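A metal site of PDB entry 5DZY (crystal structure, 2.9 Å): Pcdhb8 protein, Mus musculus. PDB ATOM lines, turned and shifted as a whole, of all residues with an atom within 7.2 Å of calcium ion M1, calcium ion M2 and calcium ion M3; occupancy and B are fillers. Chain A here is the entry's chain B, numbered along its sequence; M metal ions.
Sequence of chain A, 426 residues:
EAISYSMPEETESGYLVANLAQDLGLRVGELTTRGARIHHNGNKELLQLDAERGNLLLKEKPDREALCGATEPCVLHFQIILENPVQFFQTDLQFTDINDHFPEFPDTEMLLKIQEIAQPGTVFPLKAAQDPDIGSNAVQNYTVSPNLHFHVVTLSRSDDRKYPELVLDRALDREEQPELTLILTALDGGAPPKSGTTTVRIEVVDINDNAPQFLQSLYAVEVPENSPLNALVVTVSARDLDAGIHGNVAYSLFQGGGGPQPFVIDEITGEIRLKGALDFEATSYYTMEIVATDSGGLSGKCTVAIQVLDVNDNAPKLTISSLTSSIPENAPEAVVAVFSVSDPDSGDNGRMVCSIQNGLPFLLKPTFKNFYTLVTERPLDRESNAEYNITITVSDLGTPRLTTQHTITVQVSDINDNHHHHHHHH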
ATOM      1  N   GLU A   9      24.122 -23.426  -1.222  1.00  0.00           N
ATOM      2  CA  GLU A   9      24.026 -24.867  -1.459  1.00  0.00           C
ATOM      3  C   GLU A   9      23.731 -25.183  -2.918  1.00  0.00           C
ATOM      4  O   GLU A   9      23.307 -24.309  -3.681  1.00  0.00           O
ATOM      5  CB  GLU A   9      22.937 -25.468  -0.558  1.00  0.00           C
ATOM      6  CG  GLU A   9      22.933 -26.991  -0.468  1.00  0.00           C
ATOM      7  CD  GLU A   9      21.622 -27.542   0.037  1.00  0.00           C
ATOM      8  OE1 GLU A   9      20.753 -26.738   0.426  1.00  0.00           O
ATOM      9  OE2 GLU A   9      21.462 -28.786   0.058  1.00  0.00           O
ATOM     10  N   GLU A  10      23.979 -26.431  -3.313  1.00  0.00           N
ATOM     11  CA  GLU A  10      23.598 -26.947  -4.628  1.00  0.00           C
ATOM     12  C   GLU A  10      24.206 -26.145  -5.778  1.00  0.00           C
ATOM     13  O   GLU A  10      23.606 -26.032  -6.853  1.00  0.00           O
ATOM     14  CB  GLU A  10      22.073 -26.987  -4.771  1.00  0.00           C
ATOM     15  CG  GLU A  10      21.360 -27.828  -3.731  1.00  0.00           C
ATOM     16  CD  GLU A  10      21.523 -29.322  -3.954  1.00  0.00           C
ATOM     17  OE1 GLU A  10      22.040 -29.714  -5.016  1.00  0.00           O
ATOM     18  OE2 GLU A  10      21.136 -30.103  -3.058  1.00  0.00           O
ATOM     19  N   PRO A  62      27.531 -29.592  -3.786  1.00  0.00           N
ATOM     20  CA  PRO A  62      27.319 -29.758  -2.350  1.00  0.00           C
ATOM     21  C   PRO A  62      25.849 -29.769  -1.938  1.00  0.00           C
ATOM     22  O   PRO A  62      25.072 -28.902  -2.361  1.00  0.00           O
ATOM     23  CB  PRO A  62      28.027 -28.533  -1.766  1.00  0.00           C
ATOM     24  CG  PRO A  62      27.875 -27.488  -2.819  1.00  0.00           C
ATOM     25  CD  PRO A  62      27.916 -28.218  -4.141  1.00  0.00           C
ATOM     26  N   ASP A  63      25.481 -30.741  -1.114  1.00  0.00           N
ATOM     27  CA  ASP A  63      24.133 -30.806  -0.552  1.00  0.00           C
ATOM     28  C   ASP A  63      24.198 -30.652   0.967  1.00  0.00           C
ATOM     29  O   ASP A  63      24.705 -31.530   1.665  1.00  0.00           O
ATOM     30  CB  ASP A  63      23.450 -32.126  -0.925  1.00  0.00           C
ATOM     31  CG  ASP A  63      22.038 -32.224  -0.370  1.00  0.00           C
ATOM     32  OD1 ASP A  63      21.092 -31.823  -1.069  1.00  0.00           O
ATOM     33  OD2 ASP A  63      21.889 -32.696   0.779  1.00  0.00           O
ATOM     34  N   ARG A  64      23.694 -29.527   1.456  1.00  0.00           N
ATOM     35  CA  ARG A  64      23.766 -29.177   2.875  1.00  0.00           C
ATOM     36  C   ARG A  64      23.143 -30.252   3.757  1.00  0.00           C
ATOM     37  O   ARG A  64      23.718 -30.644   4.768  1.00  0.00           O
ATOM     38  CB  ARG A  64      23.086 -27.829   3.116  1.00  0.00           C
ATOM     39  CG  ARG A  64      23.621 -27.015   4.302  1.00  0.00           C
ATOM     40  CD  ARG A  64      23.165 -27.577   5.641  1.00  0.00           C
ATOM     41  NE  ARG A  64      21.741 -27.931   5.622  1.00  0.00           N
ATOM     42  CZ  ARG A  64      20.752 -27.106   5.942  1.00  0.00           C
ATOM     43  NH1 ARG A  64      21.027 -25.858   6.309  1.00  0.00           N
ATOM     44  NH2 ARG A  64      19.502 -27.523   5.899  1.00  0.00           N
ATOM     45  N   GLU A  65      21.968 -30.723   3.363  1.00  0.00           N
ATOM     46  CA  GLU A  65      21.240 -31.713   4.144  1.00  0.00           C
ATOM     47  C   GLU A  65      21.982 -33.045   4.216  1.00  0.00           C
ATOM     48  O   GLU A  65      21.870 -33.775   5.204  1.00  0.00           O
ATOM     49  CB  GLU A  65      19.835 -31.934   3.566  1.00  0.00           C
ATOM     50  CG  GLU A  65      18.872 -30.767   3.775  1.00  0.00           C
ATOM     51  CD  GLU A  65      19.165 -29.590   2.874  1.00  0.00           C
ATOM     52  OE1 GLU A  65      19.680 -29.807   1.753  1.00  0.00           O
ATOM     53  OE2 GLU A  65      18.890 -28.445   3.281  1.00  0.00           O
ATOM     54  N   ALA A  66      22.743 -33.347   3.182  1.00  0.00           N
ATOM     55  CA  ALA A  66      23.481 -34.612   3.115  1.00  0.00           C
ATOM     56  C   ALA A  66      24.842 -34.505   3.804  1.00  0.00           C
ATOM     57  O   ALA A  66      25.478 -35.515   4.108  1.00  0.00           O
ATOM     58  CB  ALA A  66      23.657 -35.049   1.674  1.00  0.00           C
ATOM     59  N   THR A  96      25.791 -22.116   2.586  1.00  0.00           N
ATOM     60  CA  THR A  96      24.524 -21.481   2.903  1.00  0.00           C
ATOM     61  C   THR A  96      23.363 -22.303   2.354  1.00  0.00           C
ATOM     62  O   THR A  96      23.342 -22.651   1.174  1.00  0.00           O
ATOM     63  CB  THR A  96      24.452 -20.052   2.345  1.00  0.00           C
ATOM     64  OG1 THR A  96      25.496 -19.261   2.919  1.00  0.00           O
ATOM     65  CG2 THR A  96      23.107 -19.416   2.665  1.00  0.00           C
ATOM     66  N   ASP A  97      22.390 -22.593   3.217  1.00  0.00           N
ATOM     67  CA  ASP A  97      21.244 -23.402   2.839  1.00  0.00           C
ATOM     68  C   ASP A  97      20.351 -22.694   1.819  1.00  0.00           C
ATOM     69  O   ASP A  97      20.168 -21.476   1.876  1.00  0.00           O
ATOM     70  CB  ASP A  97      20.417 -23.764   4.076  1.00  0.00           C
ATOM     71  CG  ASP A  97      19.174 -24.548   3.743  1.00  0.00           C
ATOM     72  OD1 ASP A  97      19.210 -25.351   2.789  1.00  0.00           O
ATOM     73  OD2 ASP A  97      18.140 -24.364   4.430  1.00  0.00           O
ATOM     74  N   ILE A  98      19.817 -23.467   0.878  1.00  0.00           N
ATOM     75  CA  ILE A  98      18.895 -22.945  -0.127  1.00  0.00           C
ATOM     76  C   ILE A  98      17.520 -23.595   0.045  1.00  0.00           C
ATOM     77  O   ILE A  98      17.415 -24.748   0.469  1.00  0.00           O
ATOM     78  CB  ILE A  98      19.430 -23.175  -1.555  1.00  0.00           C
ATOM     79  CG1 ILE A  98      18.568 -22.438  -2.593  1.00  0.00           C
ATOM     80  CG2 ILE A  98      19.510 -24.667  -1.873  1.00  0.00           C
ATOM     81  CD1 ILE A  98      18.516 -20.942  -2.374  1.00  0.00           C
ATOM     82  N   ASN A  99      16.462 -22.837  -0.257  1.00  0.00           N
ATOM     83  CA  ASN A  99      15.106 -23.348  -0.166  1.00  0.00           C
ATOM     84  C   ASN A  99      14.785 -24.308  -1.313  1.00  0.00           C
ATOM     85  O   ASN A  99      14.156 -23.914  -2.294  1.00  0.00           O
ATOM     86  CB  ASN A  99      14.106 -22.190  -0.148  1.00  0.00           C
ATOM     87  CG  ASN A  99      12.672 -22.661   0.056  1.00  0.00           C
ATOM     88  OD1 ASN A  99      12.427 -23.742   0.597  1.00  0.00           O
ATOM     89  ND2 ASN A  99      11.723 -21.849  -0.393  1.00  0.00           N
ATOM     90  N   ASP A 100      15.207 -25.555  -1.180  1.00  0.00           N
ATOM     91  CA  ASP A 100      15.037 -26.538  -2.242  1.00  0.00           C
ATOM     92  C   ASP A 100      14.243 -27.757  -1.788  1.00  0.00           C
ATOM     93  O   ASP A 100      14.368 -28.840  -2.353  1.00  0.00           O
ATOM     94  CB  ASP A 100      16.404 -26.987  -2.773  1.00  0.00           C
ATOM     95  CG  ASP A 100      17.275 -27.599  -1.706  1.00  0.00           C
ATOM     96  OD1 ASP A 100      17.013 -27.360  -0.504  1.00  0.00           O
ATOM     97  OD2 ASP A 100      18.228 -28.335  -2.057  1.00  0.00           O
ATOM     98  N   HIS A 101      13.412 -27.575  -0.766  1.00  0.00           N
ATOM     99  CA  HIS A 101      12.566 -28.650  -0.259  1.00  0.00           C
ATOM    100  C   HIS A 101      11.120 -28.217  -0.073  1.00  0.00           C
ATOM    101  O   HIS A 101      10.848 -27.156   0.485  1.00  0.00           O
ATOM    102  CB  HIS A 101      13.126 -29.194   1.062  1.00  0.00           C
ATOM    103  CG  HIS A 101      14.258 -30.155   0.897  1.00  0.00           C
ATOM    104  ND1 HIS A 101      15.580 -29.780   1.039  1.00  0.00           N
ATOM    105  CD2 HIS A 101      14.271 -31.471   0.617  1.00  0.00           C
ATOM    106  CE1 HIS A 101      16.353 -30.838   0.843  1.00  0.00           C
ATOM    107  NE2 HIS A 101      15.581 -31.873   0.583  1.00  0.00           N
ATOM    108  N   PHE A 102      10.200 -29.056  -0.537  1.00  0.00           N
ATOM    109  CA  PHE A 102       8.776 -28.814  -0.350  1.00  0.00           C
ATOM    110  C   PHE A 102       8.321 -29.317   1.015  1.00  0.00           C
ATOM    111  O   PHE A 102       8.714 -30.411   1.433  1.00  0.00           O
ATOM    112  CB  PHE A 102       7.956 -29.496  -1.454  1.00  0.00           C
ATOM    113  CG  PHE A 102       8.154 -28.908  -2.815  1.00  0.00           C
ATOM    114  CD1 PHE A 102       8.514 -27.584  -2.969  1.00  0.00           C
ATOM    115  CD2 PHE A 102       7.954 -29.676  -3.952  1.00  0.00           C
ATOM    116  CE1 PHE A 102       8.688 -27.036  -4.237  1.00  0.00           C
ATOM    117  CE2 PHE A 102       8.123 -29.138  -5.211  1.00  0.00           C
ATOM    118  CZ  PHE A 102       8.490 -27.818  -5.353  1.00  0.00           C
ATOM    119  N   PRO A 103       7.509 -28.520   1.720  1.00  0.00           N
ATOM    120  CA  PRO A 103       6.909 -28.970   2.980  1.00  0.00           C
ATOM    121  C   PRO A 103       6.024 -30.187   2.776  1.00  0.00           C
ATOM    122  O   PRO A 103       5.142 -30.163   1.919  1.00  0.00           O
ATOM    123  CB  PRO A 103       6.082 -27.759   3.434  1.00  0.00           C
ATOM    124  CG  PRO A 103       6.714 -26.590   2.748  1.00  0.00           C
ATOM    125  CD  PRO A 103       7.186 -27.111   1.425  1.00  0.00           C
ATOM    126  N   GLN A 130       6.900 -31.411   7.599  1.00  0.00           N
ATOM    127  CA  GLN A 130       8.344 -31.577   7.714  1.00  0.00           C
ATOM    128  C   GLN A 130       9.104 -30.766   6.664  1.00  0.00           C
ATOM    129  O   GLN A 130       8.660 -30.635   5.522  1.00  0.00           O
ATOM    130  CB  GLN A 130       8.716 -33.059   7.593  1.00  0.00           C
ATOM    131  CG  GLN A 130       8.217 -33.924   8.730  1.00  0.00           C
ATOM    132  CD  GLN A 130       8.628 -35.374   8.588  1.00  0.00           C
ATOM    133  OE1 GLN A 130       9.045 -35.806   7.513  1.00  0.00           O
ATOM    134  NE2 GLN A 130       8.512 -36.121   9.675  1.00  0.00           N
ATOM    135  N   ASP A 131      10.229 -30.205   7.069  1.00  0.00           N
ATOM    136  CA  ASP A 131      11.073 -29.416   6.175  1.00  0.00           C
ATOM    137  C   ASP A 131      12.512 -29.434   6.667  1.00  0.00           C
ATOM    138  O   ASP A 131      12.827 -28.821   7.688  1.00  0.00           O
ATOM    139  CB  ASP A 131      10.555 -27.985   6.072  1.00  0.00           C
ATOM    140  CG  ASP A 131      11.070 -27.265   4.834  1.00  0.00           C
ATOM    141  OD1 ASP A 131      12.162 -27.620   4.344  1.00  0.00           O
ATOM    142  OD2 ASP A 131      10.376 -26.337   4.356  1.00  0.00           O
ATOM    143  N   PRO A 132      13.398 -30.145   5.944  1.00  0.00           N
ATOM    144  CA  PRO A 132      14.801 -30.288   6.330  1.00  0.00           C
ATOM    145  C   PRO A 132      15.610 -28.990   6.191  1.00  0.00           C
ATOM    146  O   PRO A 132      16.763 -28.941   6.621  1.00  0.00           O
ATOM    147  CB  PRO A 132      15.325 -31.349   5.362  1.00  0.00           C
ATOM    148  CG  PRO A 132      14.461 -31.214   4.159  1.00  0.00           C
ATOM    149  CD  PRO A 132      13.100 -30.846   4.689  1.00  0.00           C
ATOM    150  N   ASP A 133      14.998 -27.968   5.600  1.00  0.00           N
ATOM    151  CA  ASP A 133      15.646 -26.673   5.459  1.00  0.00           C
ATOM    152  C   ASP A 133      15.759 -25.969   6.803  1.00  0.00           C
ATOM    153  O   ASP A 133      15.221 -26.446   7.811  1.00  0.00           O
ATOM    154  CB  ASP A 133      14.889 -25.794   4.468  1.00  0.00           C
ATOM    155  CG  ASP A 133      14.769 -26.431   3.097  1.00  0.00           C
ATOM    156  OD1 ASP A 133      15.691 -27.177   2.702  1.00  0.00           O
ATOM    157  OD2 ASP A 133      13.757 -26.178   2.403  1.00  0.00           O
ATOM    158  N   ILE A 134      16.451 -24.837   6.834  1.00  0.00           N
ATOM    159  CA  ILE A 134      16.651 -24.094   8.073  1.00  0.00           C
ATOM    160  C   ILE A 134      16.232 -22.635   7.929  1.00  0.00           C
ATOM    161  O   ILE A 134      16.061 -22.124   6.822  1.00  0.00           O
ATOM    162  CB  ILE A 134      18.121 -24.159   8.535  1.00  0.00           C
ATOM    163  CG1 ILE A 134      19.062 -23.660   7.430  1.00  0.00           C
ATOM    164  CG2 ILE A 134      18.492 -25.578   8.942  1.00  0.00           C
ATOM    165  CD1 ILE A 134      19.555 -22.232   7.631  1.00  0.00           C
ATOM    166  N   SER A 136      14.536 -19.266   7.459  1.00  0.00           N
ATOM    167  CA  SER A 136      13.368 -18.786   6.741  1.00  0.00           C
ATOM    168  C   SER A 136      12.896 -19.785   5.685  1.00  0.00           C
ATOM    169  O   SER A 136      11.782 -19.686   5.173  1.00  0.00           O
ATOM    170  CB  SER A 136      13.665 -17.435   6.087  1.00  0.00           C
ATOM    171  OG  SER A 136      12.546 -16.953   5.375  1.00  0.00           O
ATOM    172  N   ASN A 137      13.751 -20.750   5.377  1.00  0.00           N
ATOM    173  CA  ASN A 137      13.444 -21.741   4.356  1.00  0.00           C
ATOM    174  C   ASN A 137      12.647 -22.925   4.888  1.00  0.00           C
ATOM    175  O   ASN A 137      12.320 -23.853   4.155  1.00  0.00           O
ATOM    176  CB  ASN A 137      14.731 -22.242   3.688  1.00  0.00           C
ATOM    177  CG  ASN A 137      15.462 -21.155   2.933  1.00  0.00           C
ATOM    178  OD1 ASN A 137      14.845 -20.213   2.432  1.00  0.00           O
ATOM    179  ND2 ASN A 137      16.779 -21.270   2.841  1.00  0.00           N
ATOM    180  N   ALA A 138      12.341 -22.890   6.183  1.00  0.00           N
ATOM    181  CA  ALA A 138      11.549 -23.947   6.806  1.00  0.00           C
ATOM    182  C   ALA A 138      10.079 -23.566   6.874  1.00  0.00           C
ATOM    183  O   ALA A 138       9.674 -22.532   6.337  1.00  0.00           O
ATOM    184  CB  ALA A 138      12.076 -24.247   8.196  1.00  0.00           C
ATOM    185  N   VAL A 139       9.270 -24.407   7.517  1.00  0.00           N
ATOM    186  CA  VAL A 139       7.848 -24.128   7.680  1.00  0.00           C
ATOM    187  C   VAL A 139       7.630 -22.873   8.503  1.00  0.00           C
ATOM    188  O   VAL A 139       8.140 -22.746   9.621  1.00  0.00           O
ATOM    189  CB  VAL A 139       7.113 -25.310   8.337  1.00  0.00           C
ATOM    190  CG1 VAL A 139       6.794 -26.386   7.299  1.00  0.00           C
ATOM    191  CG2 VAL A 139       7.936 -25.898   9.480  1.00  0.00           C
ATOM    192  N   ASP A 188       5.987 -22.028   3.231  1.00  0.00           N
ATOM    193  CA  ASP A 188       7.374 -21.692   3.509  1.00  0.00           C
ATOM    194  C   ASP A 188       7.543 -20.172   3.585  1.00  0.00           C
ATOM    195  O   ASP A 188       6.663 -19.427   3.153  1.00  0.00           O
ATOM    196  CB  ASP A 188       8.298 -22.283   2.438  1.00  0.00           C
ATOM    197  CG  ASP A 188       9.751 -22.347   2.868  1.00  0.00           C
ATOM    198  OD1 ASP A 188      10.180 -21.522   3.690  1.00  0.00           O
ATOM    199  OD2 ASP A 188      10.472 -23.245   2.369  1.00  0.00           O
ATOM    200  N   GLY A 189       8.674 -19.723   4.131  1.00  0.00           N
ATOM    201  CA  GLY A 189       8.957 -18.307   4.230  1.00  0.00           C
ATOM    202  C   GLY A 189       9.964 -17.840   3.196  1.00  0.00           C
ATOM    203  O   GLY A 189      10.275 -16.653   3.107  1.00  0.00           O
ATOM    204  N   GLY A 190      10.470 -18.781   2.406  1.00  0.00           N
ATOM    205  CA  GLY A 190      11.432 -18.467   1.372  1.00  0.00           C
ATOM    206  C   GLY A 190      10.789 -17.738   0.199  1.00  0.00           C
ATOM    207  O   GLY A 190       9.577 -17.560   0.166  1.00  0.00           O
ATOM    208  N   LYS A 194       6.851 -22.082  -0.692  1.00  0.00           N
ATOM    209  CA  LYS A 194       6.504 -23.418  -1.176  1.00  0.00           C
ATOM    210  C   LYS A 194       5.462 -24.068  -0.273  1.00  0.00           C
ATOM    211  O   LYS A 194       5.594 -24.054   0.952  1.00  0.00           O
ATOM    212  CB  LYS A 194       7.761 -24.280  -1.274  1.00  0.00           C
ATOM    213  CG  LYS A 194       8.802 -23.720  -2.243  1.00  0.00           C
ATOM    214  CD  LYS A 194      10.092 -24.526  -2.227  1.00  0.00           C
ATOM    215  CE  LYS A 194      11.053 -24.037  -3.296  1.00  0.00           C
ATOM    216  NZ  LYS A 194      12.301 -24.843  -3.341  1.00  0.00           N
HETATM  217 CA    CA M   1      19.406 -29.837  -0.741  1.00  0.00          CA
HETATM  218 CA    CA M   2      18.068 -27.105   1.644  1.00  0.00          CA
HETATM  219 CA    CA M   3      11.368 -25.375   2.131  1.00  0.00          CA
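Of the 28 residues printed, 7 come within 4 Å of calcium ion M2.
The nearest printed residue that does not touch calcium ion M2 is Arg 64 (4.5 Å).
Six residues have an atom within 4 Å of calcium ion M3: Asn 99, His 101, Asp 131, Asp 133, Asn 137 and Asp 188.
The nearest printed residue that does not touch calcium ion M3 is Pro 103 (4.6 Å).
NH2 of Arg 64 sits close to OE2 of Glu 65, at 2.8 Å.
A ring nitrogen (ND1) of His 101 lies close to the side-chain carboxylate (OD1) of Asp 100, at 3.2 Å.
N of Asp 188 sits at hydrogen-bond distance from O of Lys 194 (3.1 Å).
The side-chain carboxylate (OD1) of Asp 188 is in hydrogen-bond range of the backbone NH (N) of Gly 190 (3.0 Å).
The side-chain carboxylate (OD2) of Asp 97 lies within salt-bridge range of the guanidinium group (NH2) of Arg 64 (3.7 Å).
N of Ile 98 lies close to OE1 of Glu 9 (3.4 Å).
O of Thr 96 lies within hydrogen-bond range of N of Glu 9, 2.6 Å away.
The side-chain carboxylate (OD1) of Asp 63 lies close to the side-chain carboxylate (OE2) of Glu 10, 2.6 Å away.
Calcium ion M2 is bound by OE2 of Glu 65, at 2.3 Å.
The side-chain carboxylate (OD1) of Asp 97 is bound to calcium ion M2, 2.4 Å away.
OD1 of Asp 100 binds calcium ion M2, at 2.4 Å.
OD1 of Asp 133 binds calcium ion M2 (2.6 Å).
Calcium ion M2 is bound by O of Ile 98 (2.7 Å).
Slightly farther from calcium ion M2 lies OE1 of Glu 9 (3.0 Å).
Slightly farther from calcium ion M2 lies OE1 of Glu 65 (3.1 Å).
Of the 28 residues printed, 6 come within 4 Å of calcium ion M1.
Calcium ion M3 is bound by the side-chain carboxylate (OD2) of Asp 188, at 2.3 Å.
Calcium ion M3 is bound by the side-chain amide oxygen (OD1) of Asn 99, at 2.5 Å.
O of His 101 binds calcium ion M3 (2.5 Å).
OD2 of Asp 133 is bound to calcium ion M3 (2.5 Å).
Calcium ion M3 is bound by the side-chain carboxylate (OD2) of Asp 131 (2.6 Å).
O of Asn 137 binds calcium ion M3 (2.7 Å).
Calcium ion M3 has six donor atoms within binding distance.
Calcium ion M1 is bound by the side-chain carboxylate of Asp 100 (2.3 Å), the side-chain carboxylate of Glu 9 (2.4 Å), the side-chain carboxylate of Glu 65 (2.5 Å) and the side-chain carboxylate of Asp 63 (2.6 Å).
Calcium ion M1 has four donor atoms within binding distance.
Slightly farther from calcium ion M1 lies OE2 of Glu 10 (2.9 Å).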
